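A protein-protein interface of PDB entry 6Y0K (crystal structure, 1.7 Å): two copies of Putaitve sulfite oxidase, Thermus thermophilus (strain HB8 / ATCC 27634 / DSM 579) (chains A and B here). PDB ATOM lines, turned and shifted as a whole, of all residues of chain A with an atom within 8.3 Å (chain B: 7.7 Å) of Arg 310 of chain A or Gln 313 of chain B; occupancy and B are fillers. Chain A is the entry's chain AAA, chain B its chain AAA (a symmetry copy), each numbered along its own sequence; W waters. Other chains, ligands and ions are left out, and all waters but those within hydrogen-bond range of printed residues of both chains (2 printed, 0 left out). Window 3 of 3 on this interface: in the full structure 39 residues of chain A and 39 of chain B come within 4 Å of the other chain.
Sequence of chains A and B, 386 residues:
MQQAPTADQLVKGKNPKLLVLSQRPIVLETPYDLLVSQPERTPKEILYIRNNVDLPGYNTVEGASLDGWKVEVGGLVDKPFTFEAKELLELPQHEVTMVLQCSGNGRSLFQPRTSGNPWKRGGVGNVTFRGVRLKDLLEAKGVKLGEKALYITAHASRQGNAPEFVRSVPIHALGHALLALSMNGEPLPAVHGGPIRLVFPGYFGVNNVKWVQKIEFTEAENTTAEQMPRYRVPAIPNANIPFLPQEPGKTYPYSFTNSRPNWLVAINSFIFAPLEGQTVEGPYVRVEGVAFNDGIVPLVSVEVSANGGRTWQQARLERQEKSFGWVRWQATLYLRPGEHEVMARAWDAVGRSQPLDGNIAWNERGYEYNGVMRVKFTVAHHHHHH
Of chain B, only Gln 313 (3.7 Å) and Gln 314 (2.9 Å) come within 4 Å of Arg 310 of chain A.
Of chain A, only Arg 310 (3.7 Å) comes within 4 Å of Gln 313 of chain B.
Of the printed residues of chain B, Gly 309 of chain A touches Gln 314.
Printed residues of chain A within 4 Å of Glu 303 of chain B: Trp 312 and Arg 345.
Of the printed residues of chain B, Thr 311 of chain A touches Trp 312.
Of the printed residues of chain A, Gln 314 of chain B touches Gly 309 and Arg 310.
Of the printed residues of chain A, Thr 311 of chain B touches Trp 312.
Ser 301 of chain B touches none of the printed residues of chain A.
Val 304 of chain B touches none of the printed residues of chain A.
The nearest residue of chain B that does not touch Arg 310 of chain A is Trp 312 of chain B (4.1 Å).
Among the printed residues, merely in contact across the chains: Glu 303 of chain A with Trp 312 of chain B, Gly 309 of chain A with Gln 314 of chain B, Arg 310 of chain A with Gln 313 of chain B, Thr 311 of chain A with Trp 312 of chain B, Trp 312 of chain A with Glu 303 of chain B and Trp 312 of chain A with Thr 311 of chain B.
The side-chain carboxylate of Glu 303 of chain A is in salt-bridge range of the guanidinium group of Arg 345 of chain B (2.6 Å).
O of Arg 310 of chain A lies within hydrogen-bond range of N of Gln 314 of chain B (2.9 Å).
The backbone NH (N) of Trp 312 of chain B is in hydrogen-bond range of the backbone carbonyl oxygen (O) of Trp 312 of chain A (2.9 Å).
The side-chain carboxylate (OE1) of Glu 303 of chain B is in salt-bridge range of the guanidinium group (NH2) of Arg 345 of chain A (2.6 Å).
The guanidinium group (NH2) of Arg 345 of chain A lies close to the guanidinium group (NH2) of Arg 345 of chain B, 2.2 Å away.
Water W2 lies within hydrogen-bond range of OE2 of Glu 303 of chain B (2.6 Å), O of Gly 309 of chain A (2.7 Å), NE1 of Trp 312 of chain A (3.1 Å) and NE2 of Gln 314 of chain B (3.5 Å).
Water W1 bridges the side-chain carboxylate (OE2) of Glu 303 of chain A and the indole nitrogen (NE1) of Trp 312 of chain B.
Glu 303 of chain A touches Trp 312 of chain B, and with the chains exchanged Trp 312 of chain A touches Glu 303 of chain B.
Thr 311 of chain A touches Trp 312 of chain B, and with the chains exchanged Trp 312 of chain A touches Thr 311 of chain B.
Trp 312 of chain A touches its own counterpart, Trp 312 of chain B.
Arg 345 of chain A touches its own counterpart, Arg 345 of chain B.
N of Gly 309 of chain A lies within hydrogen-bond range of OG of Ser 305 of chain A (2.8 Å).
The side-chain amide oxygen (OD1) of Asn 307 of chain A is in hydrogen-bond range of the backbone NH (N) of Arg 310 of chain A, 3.1 Å away.
The side-chain hydroxyl of Ser 301 of chain B sits at hydrogen-bond distance from the side-chain carboxylate of Glu 303 of chain B (2.7 Å).
OE1 of Glu 303 of chain B lies within salt-bridge range of NH2 of Arg 345 of chain B (2.9 Å).
The side-chain amide nitrogen of Asn 307 of chain B is in hydrogen-bond range of the side-chain hydroxyl of Thr 311 of chain B.
Printed residues of chain A that touch a printed residue of chain B: Glu 303, Gly 309, Arg 310, Thr 311, Trp 312 and Arg 345.
Hydrophobic or aromatic side chains of chain A that line the printed part of chain B: Trp 312.
Among the printed residues, 11 pairs touch across the chains.
Among the printed residues, Asp or Glu carboxylates within 4 Å of a Lys or Arg side-chain nitrogen of the other chain: Glu 303 of chain A with Arg 345 of chain B (2.6 Å) and Arg 345 of chain A with Glu 303 of chain B (2.6 Å).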
ATOM      1  N   GLU A 303      -7.322 -22.059  29.059  1.00  0.00           N
ATOM      2  CA  GLU A 303      -8.484 -22.958  29.249  1.00  0.00           C
ATOM      3  C   GLU A 303      -7.987 -24.381  29.072  1.00  0.00           C
ATOM      4  O   GLU A 303      -7.000 -24.602  28.349  1.00  0.00           O
ATOM      5  CB  GLU A 303      -9.623 -22.580  28.305  1.00  0.00           C
ATOM      6  CG  GLU A 303     -10.081 -21.142  28.478  1.00  0.00           C
ATOM      7  CD  GLU A 303     -10.968 -20.650  27.352  1.00  0.00           C
ATOM      8  OE1 GLU A 303     -11.325 -21.486  26.514  1.00  0.00           O
ATOM      9  OE2 GLU A 303     -11.304 -19.437  27.320  1.00  0.00           O
ATOM     10  N   VAL A 304      -8.608 -25.307  29.788  1.00  0.00           N
ATOM     11  CA  VAL A 304      -8.245 -26.739  29.733  1.00  0.00           C
ATOM     12  C   VAL A 304      -9.509 -27.521  29.397  1.00  0.00           C
ATOM     13  O   VAL A 304     -10.632 -27.088  29.756  1.00  0.00           O
ATOM     14  CB  VAL A 304      -7.595 -27.225  31.031  1.00  0.00           C
ATOM     15  CG1 VAL A 304      -6.328 -26.446  31.358  1.00  0.00           C
ATOM     16  CG2 VAL A 304      -8.575 -27.181  32.179  1.00  0.00           C
ATOM     17  N   SER A 305      -9.325 -28.617  28.683  1.00  0.00           N
ATOM     18  CA  SER A 305     -10.405 -29.565  28.348  1.00  0.00           C
ATOM     19  C   SER A 305      -9.912 -30.957  28.704  1.00  0.00           C
ATOM     20  O   SER A 305      -8.721 -31.244  28.432  1.00  0.00           O
ATOM     21  CB  SER A 305     -10.792 -29.480  26.908  1.00  0.00           C
ATOM     22  OG  SER A 305     -11.854 -30.373  26.633  1.00  0.00           O
ATOM     23  N   ALA A 306     -10.774 -31.749  29.343  1.00  0.00           N
ATOM     24  CA  ALA A 306     -10.518 -33.171  29.648  1.00  0.00           C
ATOM     25  C   ALA A 306     -11.482 -34.047  28.849  1.00  0.00           C
ATOM     26  O   ALA A 306     -11.449 -35.272  29.067  1.00  0.00           O
ATOM     27  CB  ALA A 306     -10.659 -33.413  31.139  1.00  0.00           C
ATOM     28  N   ASN A 307     -12.273 -33.461  27.940  1.00  0.00           N
ATOM     29  CA  ASN A 307     -13.302 -34.205  27.162  1.00  0.00           C
ATOM     30  C   ASN A 307     -13.150 -33.910  25.664  1.00  0.00           C
ATOM     31  O   ASN A 307     -14.182 -33.837  24.968  1.00  0.00           O
ATOM     32  CB  ASN A 307     -14.700 -33.908  27.703  1.00  0.00           C
ATOM     33  CG  ASN A 307     -15.111 -32.458  27.563  1.00  0.00           C
ATOM     34  OD1 ASN A 307     -14.466 -31.670  26.864  1.00  0.00           O
ATOM     35  ND2 ASN A 307     -16.201 -32.102  28.212  1.00  0.00           N
ATOM     36  N   GLY A 308     -11.908 -33.765  25.194  1.00  0.00           N
ATOM     37  CA  GLY A 308     -11.557 -33.595  23.773  1.00  0.00           C
ATOM     38  C   GLY A 308     -12.115 -32.313  23.175  1.00  0.00           C
ATOM     39  O   GLY A 308     -12.375 -32.319  21.958  1.00  0.00           O
ATOM     40  N   GLY A 309     -12.312 -31.262  23.980  1.00  0.00           N
ATOM     41  CA  GLY A 309     -12.732 -29.934  23.488  1.00  0.00           C
ATOM     42  C   GLY A 309     -14.235 -29.715  23.496  1.00  0.00           C
ATOM     43  O   GLY A 309     -14.668 -28.603  23.094  1.00  0.00           O
ATOM     44  N   ARG A 310     -15.028 -30.681  23.964  1.00  0.00           N
ATOM     45  CA  ARG A 310     -16.502 -30.508  24.075  1.00  0.00           C
ATOM     46  C   ARG A 310     -16.772 -29.364  25.061  1.00  0.00           C
ATOM     47  O   ARG A 310     -17.692 -28.559  24.802  1.00  0.00           O
ATOM     48  CB  ARG A 310     -17.201 -31.818  24.468  1.00  0.00           C
ATOM     49  CG  ARG A 310     -17.062 -32.924  23.425  1.00  0.00           C
ATOM     50  CD  ARG A 310     -17.939 -34.159  23.639  1.00  0.00           C
ATOM     51  NE  ARG A 310     -17.679 -34.870  24.892  1.00  0.00           N
ATOM     52  CZ  ARG A 310     -18.322 -34.678  26.052  1.00  0.00           C
ATOM     53  NH1 ARG A 310     -19.297 -33.784  26.151  1.00  0.00           N
ATOM     54  NH2 ARG A 310     -17.978 -35.384  27.121  1.00  0.00           N
ATOM     55  N   THR A 311     -15.989 -29.271  26.137  1.00  0.00           N
ATOM     56  CA  THR A 311     -16.061 -28.139  27.097  1.00  0.00           C
ATOM     57  C   THR A 311     -14.640 -27.687  27.439  1.00  0.00           C
ATOM     58  O   THR A 311     -13.757 -28.547  27.589  1.00  0.00           O
ATOM     59  CB  THR A 311     -16.865 -28.490  28.357  1.00  0.00           C
ATOM     60  OG1 THR A 311     -16.107 -29.464  29.065  1.00  0.00           O
ATOM     61  CG2 THR A 311     -18.244 -29.031  28.046  1.00  0.00           C
ATOM     62  N   TRP A 312     -14.454 -26.370  27.524  1.00  0.00           N
ATOM     63  CA  TRP A 312     -13.200 -25.722  27.978  1.00  0.00           C
ATOM     64  C   TRP A 312     -13.482 -24.978  29.287  1.00  0.00           C
ATOM     65  O   TRP A 312     -14.500 -24.267  29.350  1.00  0.00           O
ATOM     66  CB  TRP A 312     -12.670 -24.797  26.883  1.00  0.00           C
ATOM     67  CG  TRP A 312     -12.193 -25.544  25.676  1.00  0.00           C
ATOM     68  CD1 TRP A 312     -12.932 -25.915  24.588  1.00  0.00           C
ATOM     69  CD2 TRP A 312     -10.853 -25.998  25.429  1.00  0.00           C
ATOM     70  NE1 TRP A 312     -12.141 -26.559  23.672  1.00  0.00           N
ATOM     71  CE2 TRP A 312     -10.859 -26.623  24.161  1.00  0.00           C
ATOM     72  CE3 TRP A 312      -9.647 -25.918  26.140  1.00  0.00           C
ATOM     73  CZ2 TRP A 312      -9.707 -27.162  23.602  1.00  0.00           C
ATOM     74  CZ3 TRP A 312      -8.508 -26.457  25.585  1.00  0.00           C
ATOM     75  CH2 TRP A 312      -8.556 -27.105  24.350  1.00  0.00           C
ATOM     76  N   GLN A 313     -12.610 -25.155  30.276  1.00  0.00           N
ATOM     77  CA  GLN A 313     -12.717 -24.563  31.635  1.00  0.00           C
ATOM     78  C   GLN A 313     -11.616 -23.522  31.797  1.00  0.00           C
ATOM     79  O   GLN A 313     -10.449 -23.892  31.584  1.00  0.00           O
ATOM     80  CB  GLN A 313     -12.483 -25.611  32.718  1.00  0.00           C
ATOM     81  CG  GLN A 313     -13.709 -26.404  33.112  1.00  0.00           C
ATOM     82  CD  GLN A 313     -13.379 -27.281  34.293  1.00  0.00           C
ATOM     83  OE1 GLN A 313     -13.541 -28.497  34.242  1.00  0.00           O
ATOM     84  NE2 GLN A 313     -12.874 -26.666  35.355  1.00  0.00           N
ATOM     85  N   MET A 343      -5.954 -31.078  27.611  1.00  0.00           N
ATOM     86  CA  MET A 343      -5.447 -30.154  26.572  1.00  0.00           C
ATOM     87  C   MET A 343      -5.465 -28.758  27.180  1.00  0.00           C
ATOM     88  O   MET A 343      -6.402 -28.477  27.943  1.00  0.00           O
ATOM     89  CB  MET A 343      -6.393 -30.105  25.375  1.00  0.00           C
ATOM     90  CG  MET A 343      -6.735 -31.420  24.776  1.00  0.00           C
ATOM     91  SD  MET A 343      -7.553 -31.053  23.206  1.00  0.00           S
ATOM     92  CE  MET A 343      -9.242 -30.952  23.776  1.00  0.00           C
ATOM     93  N   ARG A 345      -5.217 -24.447  26.098  1.00  0.00           N
ATOM     94  CA  ARG A 345      -5.165 -23.420  25.028  1.00  0.00           C
ATOM     95  C   ARG A 345      -5.150 -22.032  25.653  1.00  0.00           C
ATOM     96  O   ARG A 345      -5.917 -21.774  26.595  1.00  0.00           O
ATOM     97  CB  ARG A 345      -6.291 -23.632  24.020  1.00  0.00           C
ATOM     98  CG  ARG A 345      -7.646 -23.118  24.448  1.00  0.00           C
ATOM     99  CD  ARG A 345      -8.626 -23.150  23.301  1.00  0.00           C
ATOM    100  NE  ARG A 345      -9.906 -22.858  23.914  1.00  0.00           N
ATOM    101  CZ  ARG A 345     -11.082 -23.157  23.407  1.00  0.00           C
ATOM    102  NH1 ARG A 345     -11.185 -23.767  22.244  1.00  0.00           N
ATOM    103  NH2 ARG A 345     -12.165 -22.843  24.085  1.00  0.00           N
ATOM    104  N   SER B 301     -14.196 -24.917  15.871  1.00  0.00           N
ATOM    105  CA  SER B 301     -15.363 -24.885  16.784  1.00  0.00           C
ATOM    106  C   SER B 301     -16.047 -23.533  16.733  1.00  0.00           C
ATOM    107  O   SER B 301     -15.379 -22.523  16.463  1.00  0.00           O
ATOM    108  CB  SER B 301     -14.951 -25.207  18.195  1.00  0.00           C
ATOM    109  OG  SER B 301     -14.232 -24.128  18.783  1.00  0.00           O
ATOM    110  N   VAL B 302     -17.331 -23.531  17.053  1.00  0.00           N
ATOM    111  CA  VAL B 302     -18.027 -22.350  17.622  1.00  0.00           C
ATOM    112  C   VAL B 302     -18.429 -22.746  19.035  1.00  0.00           C
ATOM    113  O   VAL B 302     -18.932 -23.878  19.207  1.00  0.00           O
ATOM    114  CB  VAL B 302     -19.228 -21.918  16.775  1.00  0.00           C
ATOM    115  CG1 VAL B 302     -19.962 -20.753  17.421  1.00  0.00           C
ATOM    116  CG2 VAL B 302     -18.786 -21.580  15.367  1.00  0.00           C
ATOM    117  N   GLU B 303     -18.158 -21.889  20.010  1.00  0.00           N
ATOM    118  CA  GLU B 303     -18.366 -22.219  21.439  1.00  0.00           C
ATOM    119  C   GLU B 303     -19.220 -21.117  22.037  1.00  0.00           C
ATOM    120  O   GLU B 303     -19.180 -19.974  21.548  1.00  0.00           O
ATOM    121  CB  GLU B 303     -17.031 -22.421  22.152  1.00  0.00           C
ATOM    122  CG  GLU B 303     -16.180 -23.507  21.515  1.00  0.00           C
ATOM    123  CD  GLU B 303     -14.741 -23.503  21.989  1.00  0.00           C
ATOM    124  OE1 GLU B 303     -14.457 -22.733  22.913  1.00  0.00           O
ATOM    125  OE2 GLU B 303     -13.912 -24.274  21.437  1.00  0.00           O
ATOM    126  N   VAL B 304     -20.036 -21.479  23.017  1.00  0.00           N
ATOM    127  CA  VAL B 304     -20.934 -20.527  23.705  1.00  0.00           C
ATOM    128  C   VAL B 304     -20.651 -20.625  25.199  1.00  0.00           C
ATOM    129  O   VAL B 304     -20.253 -21.707  25.695  1.00  0.00           O
ATOM    130  CB  VAL B 304     -22.409 -20.780  23.380  1.00  0.00           C
ATOM    131  CG1 VAL B 304     -22.688 -20.673  21.887  1.00  0.00           C
ATOM    132  CG2 VAL B 304     -22.864 -22.112  23.927  1.00  0.00           C
ATOM    133  N   SER B 305     -20.807 -19.504  25.880  1.00  0.00           N
ATOM    134  CA  SER B 305     -20.687 -19.416  27.349  1.00  0.00           C
ATOM    135  C   SER B 305     -21.916 -18.684  27.860  1.00  0.00           C
ATOM    136  O   SER B 305     -22.323 -17.694  27.206  1.00  0.00           O
ATOM    137  CB  SER B 305     -19.432 -18.723  27.763  1.00  0.00           C
ATOM    138  OG  SER B 305     -19.331 -18.693  29.173  1.00  0.00           O
ATOM    139  N   ALA B 306     -22.509 -19.197  28.939  1.00  0.00           N
ATOM    140  CA  ALA B 306     -23.627 -18.549  29.652  1.00  0.00           C
ATOM    141  C   ALA B 306     -23.168 -18.126  31.047  1.00  0.00           C
ATOM    142  O   ALA B 306     -24.027 -17.642  31.806  1.00  0.00           O
ATOM    143  CB  ALA B 306     -24.811 -19.495  29.725  1.00  0.00           C
ATOM    144  N   ASN B 307     -21.871 -18.258  31.359  1.00  0.00           N
ATOM    145  CA  ASN B 307     -21.329 -17.951  32.712  1.00  0.00           C
ATOM    146  C   ASN B 307     -20.114 -17.020  32.596  1.00  0.00           C
ATOM    147  O   ASN B 307     -19.173 -17.174  33.399  1.00  0.00           O
ATOM    148  CB  ASN B 307     -21.038 -19.240  33.478  1.00  0.00           C
ATOM    149  CG  ASN B 307     -19.967 -20.099  32.839  1.00  0.00           C
ATOM    150  OD1 ASN B 307     -19.251 -19.666  31.931  1.00  0.00           O
ATOM    151  ND2 ASN B 307     -19.838 -21.317  33.325  1.00  0.00           N
ATOM    152  N   THR B 311     -16.798 -21.231  31.560  1.00  0.00           N
ATOM    153  CA  THR B 311     -16.845 -22.469  30.740  1.00  0.00           C
ATOM    154  C   THR B 311     -17.376 -22.123  29.348  1.00  0.00           C
ATOM    155  O   THR B 311     -18.300 -21.300  29.246  1.00  0.00           O
ATOM    156  CB  THR B 311     -17.670 -23.580  31.404  1.00  0.00           C
ATOM    157  OG1 THR B 311     -19.023 -23.140  31.400  1.00  0.00           O
ATOM    158  CG2 THR B 311     -17.228 -23.878  32.821  1.00  0.00           C
ATOM    159  N   TRP B 312     -16.770 -22.730  28.327  1.00  0.00           N
ATOM    160  CA  TRP B 312     -17.212 -22.649  26.915  1.00  0.00           C
ATOM    161  C   TRP B 312     -17.654 -24.044  26.462  1.00  0.00           C
ATOM    162  O   TRP B 312     -16.922 -25.010  26.735  1.00  0.00           O
ATOM    163  CB  TRP B 312     -16.083 -22.086  26.051  1.00  0.00           C
ATOM    164  CG  TRP B 312     -15.790 -20.649  26.349  1.00  0.00           C
ATOM    165  CD1 TRP B 312     -14.917 -20.158  27.279  1.00  0.00           C
ATOM    166  CD2 TRP B 312     -16.364 -19.508  25.691  1.00  0.00           C
ATOM    167  NE1 TRP B 312     -14.899 -18.788  27.240  1.00  0.00           N
ATOM    168  CE2 TRP B 312     -15.776 -18.361  26.273  1.00  0.00           C
ATOM    169  CE3 TRP B 312     -17.296 -19.342  24.657  1.00  0.00           C
ATOM    170  CZ2 TRP B 312     -16.097 -17.077  25.850  1.00  0.00           C
ATOM    171  CZ3 TRP B 312     -17.615 -18.067  24.245  1.00  0.00           C
ATOM    172  CH2 TRP B 312     -17.049 -16.955  24.868  1.00  0.00           C
ATOM    173  N   GLN B 313     -18.811 -24.122  25.809  1.00  0.00           N
ATOM    174  CA  GLN B 313     -19.442 -25.376  25.321  1.00  0.00           C
ATOM    175  C   GLN B 313     -19.390 -25.383  23.798  1.00  0.00           C
ATOM    176  O   GLN B 313     -19.878 -24.403  23.209  1.00  0.00           O
ATOM    177  CB  GLN B 313     -20.917 -25.440  25.704  1.00  0.00           C
ATOM    178  CG  GLN B 313     -21.194 -25.995  27.082  1.00  0.00           C
ATOM    179  CD  GLN B 313     -22.681 -26.156  27.268  1.00  0.00           C
ATOM    180  OE1 GLN B 313     -23.264 -25.609  28.200  1.00  0.00           O
ATOM    181  NE2 GLN B 313     -23.310 -26.881  26.352  1.00  0.00           N
ATOM    182  N   GLN B 314     -18.900 -26.470  23.206  1.00  0.00           N
ATOM    183  CA  GLN B 314     -18.841 -26.636  21.734  1.00  0.00           C
ATOM    184  C   GLN B 314     -20.272 -26.681  21.177  1.00  0.00           C
ATOM    185  O   GLN B 314     -21.096 -27.479  21.682  1.00  0.00           O
ATOM    186  CB  GLN B 314     -18.032 -27.886  21.392  1.00  0.00           C
ATOM    187  CG  GLN B 314     -17.602 -27.947  19.939  1.00  0.00           C
ATOM    188  CD  GLN B 314     -16.666 -29.098  19.687  1.00  0.00           C
ATOM    189  OE1 GLN B 314     -16.863 -30.189  20.201  1.00  0.00           O
ATOM    190  NE2 GLN B 314     -15.635 -28.856  18.893  1.00  0.00           N
ATOM    191  N   ALA B 315     -20.571 -25.855  20.175  1.00  0.00           N
ATOM    192  CA  ALA B 315     -21.837 -25.909  19.413  1.00  0.00           C
ATOM    193  C   ALA B 315     -21.706 -26.975  18.326  1.00  0.00           C
ATOM    194  O   ALA B 315     -20.569 -27.426  18.036  1.00  0.00           O
ATOM    195  CB  ALA B 315     -22.174 -24.558  18.815  1.00  0.00           C
ATOM    196  N   ARG B 316     -22.836 -27.373  17.759  1.00  0.00           N
ATOM    197  CA  ARG B 316     -22.898 -28.262  16.567  1.00  0.00           C
ATOM    198  C   ARG B 316     -22.913 -27.385  15.312  1.00  0.00           C
ATOM    199  O   ARG B 316     -23.740 -26.479  15.248  1.00  0.00           O
ATOM    200  CB  ARG B 316     -24.147 -29.153  16.606  1.00  0.00           C
ATOM    201  CG  ARG B 316     -24.438 -29.762  17.969  1.00  0.00           C
ATOM    202  CD  ARG B 316     -23.221 -30.330  18.683  1.00  0.00           C
ATOM    203  NE  ARG B 316     -23.002 -31.738  18.375  1.00  0.00           N
ATOM    204  CZ  ARG B 316     -23.519 -32.764  19.048  1.00  0.00           C
ATOM    205  NH1 ARG B 316     -24.304 -32.565  20.097  1.00  0.00           N
ATOM    206  NH2 ARG B 316     -23.242 -33.998  18.665  1.00  0.00           N
ATOM    207  N   TRP B 329     -24.785 -22.732  13.231  1.00  0.00           N
ATOM    208  CA  TRP B 329     -24.433 -23.481  14.456  1.00  0.00           C
ATOM    209  C   TRP B 329     -25.586 -23.393  15.460  1.00  0.00           C
ATOM    210  O   TRP B 329     -26.411 -22.443  15.402  1.00  0.00           O
ATOM    211  CB  TRP B 329     -23.106 -22.979  15.050  1.00  0.00           C
ATOM    212  CG  TRP B 329     -23.075 -21.533  15.431  1.00  0.00           C
ATOM    213  CD1 TRP B 329     -22.562 -20.482  14.711  1.00  0.00           C
ATOM    214  CD2 TRP B 329     -23.589 -20.958  16.642  1.00  0.00           C
ATOM    215  NE1 TRP B 329     -22.703 -19.312  15.413  1.00  0.00           N
ATOM    216  CE2 TRP B 329     -23.341 -19.570  16.595  1.00  0.00           C
ATOM    217  CE3 TRP B 329     -24.213 -21.490  17.775  1.00  0.00           C
ATOM    218  CZ2 TRP B 329     -23.718 -18.702  17.624  1.00  0.00           C
ATOM    219  CZ3 TRP B 329     -24.583 -20.636  18.788  1.00  0.00           C
ATOM    220  CH2 TRP B 329     -24.352 -19.261  18.705  1.00  0.00           C
ATOM    221  N   GLN B 330     -25.605 -24.349  16.385  1.00  0.00           N
ATOM    222  CA  GLN B 330     -26.601 -24.386  17.489  1.00  0.00           C
ATOM    223  C   GLN B 330     -25.941 -25.027  18.702  1.00  0.00           C
ATOM    224  O   GLN B 330     -25.160 -25.959  18.528  1.00  0.00           O
ATOM    225  CB  GLN B 330     -27.866 -25.152  17.089  1.00  0.00           C
ATOM    226  CG  GLN B 330     -27.690 -26.664  17.035  1.00  0.00           C
ATOM    227  CD  GLN B 330     -27.829 -27.384  18.367  1.00  0.00           C
ATOM    228  OE1 GLN B 330     -28.056 -26.780  19.422  1.00  0.00           O
ATOM    229  NE2 GLN B 330     -27.655 -28.697  18.333  1.00  0.00           N
ATOM    230  N   ALA B 331     -26.221 -24.468  19.877  1.00  0.00           N
ATOM    231  CA  ALA B 331     -25.871 -25.046  21.189  1.00  0.00           C
ATOM    232  C   ALA B 331     -27.126 -24.989  22.046  1.00  0.00           C
ATOM    233  O   ALA B 331     -27.693 -23.894  22.216  1.00  0.00           O
ATOM    234  CB  ALA B 331     -24.727 -24.306  21.826  1.00  0.00           C
ATOM    235  N   THR B 332     -27.520 -26.139  22.578  1.00  0.00           N
ATOM    236  CA  THR B 332     -28.700 -26.243  23.461  1.00  0.00           C
ATOM    237  C   THR B 332     -28.177 -26.222  24.896  1.00  0.00           C
ATOM    238  O   THR B 332     -27.362 -27.092  25.242  1.00  0.00           O
ATOM    239  CB  THR B 332     -29.573 -27.433  23.050  1.00  0.00           C
ATOM    240  OG1 THR B 332     -29.918 -27.224  21.675  1.00  0.00           O
ATOM    241  CG2 THR B 332     -30.836 -27.524  23.871  1.00  0.00           C
ATOM    242  N   LEU B 333     -28.582 -25.212  25.655  1.00  0.00           N
ATOM    243  CA  LEU B 333     -28.102 -24.963  27.037  1.00  0.00           C
ATOM    244  C   LEU B 333     -29.244 -25.216  28.026  1.00  0.00           C
ATOM    245  O   LEU B 333     -30.349 -24.708  27.785  1.00  0.00           O
ATOM    246  CB  LEU B 333     -27.636 -23.507  27.144  1.00  0.00           C
ATOM    247  CG  LEU B 333     -26.508 -23.075  26.205  1.00  0.00           C
ATOM    248  CD1 LEU B 333     -26.046 -21.674  26.572  1.00  0.00           C
ATOM    249  CD2 LEU B 333     -25.344 -24.045  26.269  1.00  0.00           C
ATOM    250  N   TYR B 334     -28.952 -25.889  29.144  1.00  0.00           N
ATOM    251  CA  TYR B 334     -29.864 -25.981  30.317  1.00  0.00           C
ATOM    252  C   TYR B 334     -29.722 -24.693  31.134  1.00  0.00           C
ATOM    253  O   TYR B 334     -28.646 -24.464  31.705  1.00  0.00           O
ATOM    254  CB  TYR B 334     -29.551 -27.202  31.183  1.00  0.00           C
ATOM    255  CG  TYR B 334     -30.547 -27.392  32.298  1.00  0.00           C
ATOM    256  CD1 TYR B 334     -30.444 -26.683  33.488  1.00  0.00           C
ATOM    257  CD2 TYR B 334     -31.630 -28.245  32.142  1.00  0.00           C
ATOM    258  CE1 TYR B 334     -31.382 -26.832  34.499  1.00  0.00           C
ATOM    259  CE2 TYR B 334     -32.573 -28.411  33.145  1.00  0.00           C
ATOM    260  CZ  TYR B 334     -32.449 -27.701  34.325  1.00  0.00           C
ATOM    261  OH  TYR B 334     -33.381 -27.866  35.306  1.00  0.00           O
ATOM    262  N   LEU B 335     -30.755 -23.853  31.166  1.00  0.00           N
ATOM    263  CA  LEU B 335     -30.713 -22.574  31.920  1.00  0.00           C
ATOM    264  C   LEU B 335     -31.914 -22.477  32.866  1.00  0.00           C
ATOM    265  O   LEU B 335     -33.045 -22.703  32.407  1.00  0.00           O
ATOM    266  CB  LEU B 335     -30.730 -21.412  30.927  1.00  0.00           C
ATOM    267  CG  LEU B 335     -29.534 -21.337  29.979  1.00  0.00           C
ATOM    268  CD1 LEU B 335     -29.705 -20.155  29.041  1.00  0.00           C
ATOM    269  CD2 LEU B 335     -28.224 -21.226  30.748  1.00  0.00           C
ATOM    270  N   MET B 343     -22.660 -15.680  25.158  1.00  0.00           N
ATOM    271  CA  MET B 343     -21.564 -15.167  24.306  1.00  0.00           C
ATOM    272  C   MET B 343     -21.223 -16.274  23.316  1.00  0.00           C
ATOM    273  O   MET B 343     -21.278 -17.444  23.725  1.00  0.00           O
ATOM    274  CB  MET B 343     -20.298 -14.930  25.125  1.00  0.00           C
ATOM    275  CG  MET B 343     -20.465 -14.071  26.325  1.00  0.00           C
ATOM    276  SD  MET B 343     -18.794 -13.673  26.887  1.00  0.00           S
ATOM    277  CE  MET B 343     -18.526 -15.048  27.995  1.00  0.00           C
ATOM    278  N   ARG B 345     -18.100 -17.561  20.418  1.00  0.00           N
ATOM    279  CA  ARG B 345     -16.753 -17.333  19.837  1.00  0.00           C
ATOM    280  C   ARG B 345     -16.442 -18.429  18.826  1.00  0.00           C
ATOM    281  O   ARG B 345     -16.705 -19.611  19.100  1.00  0.00           O
ATOM    282  CB  ARG B 345     -15.706 -17.193  20.938  1.00  0.00           C
ATOM    283  CG  ARG B 345     -15.225 -18.491  21.543  1.00  0.00           C
ATOM    284  CD  ARG B 345     -14.030 -18.265  22.435  1.00  0.00           C
ATOM    285  NE  ARG B 345     -13.839 -19.535  23.108  1.00  0.00           N
ATOM    286  CZ  ARG B 345     -13.192 -19.710  24.239  1.00  0.00           C
ATOM    287  NH1 ARG B 345     -12.637 -18.694  24.868  1.00  0.00           N
ATOM    288  NH2 ARG B 345     -13.111 -20.922  24.743  1.00  0.00           N
HETATM  289  O   HOH W   1     -12.547 -17.909  29.056  1.00  0.00           O
HETATM  290  O   HOH W   2     -13.870 -26.879  21.120  1.00  0.00           O
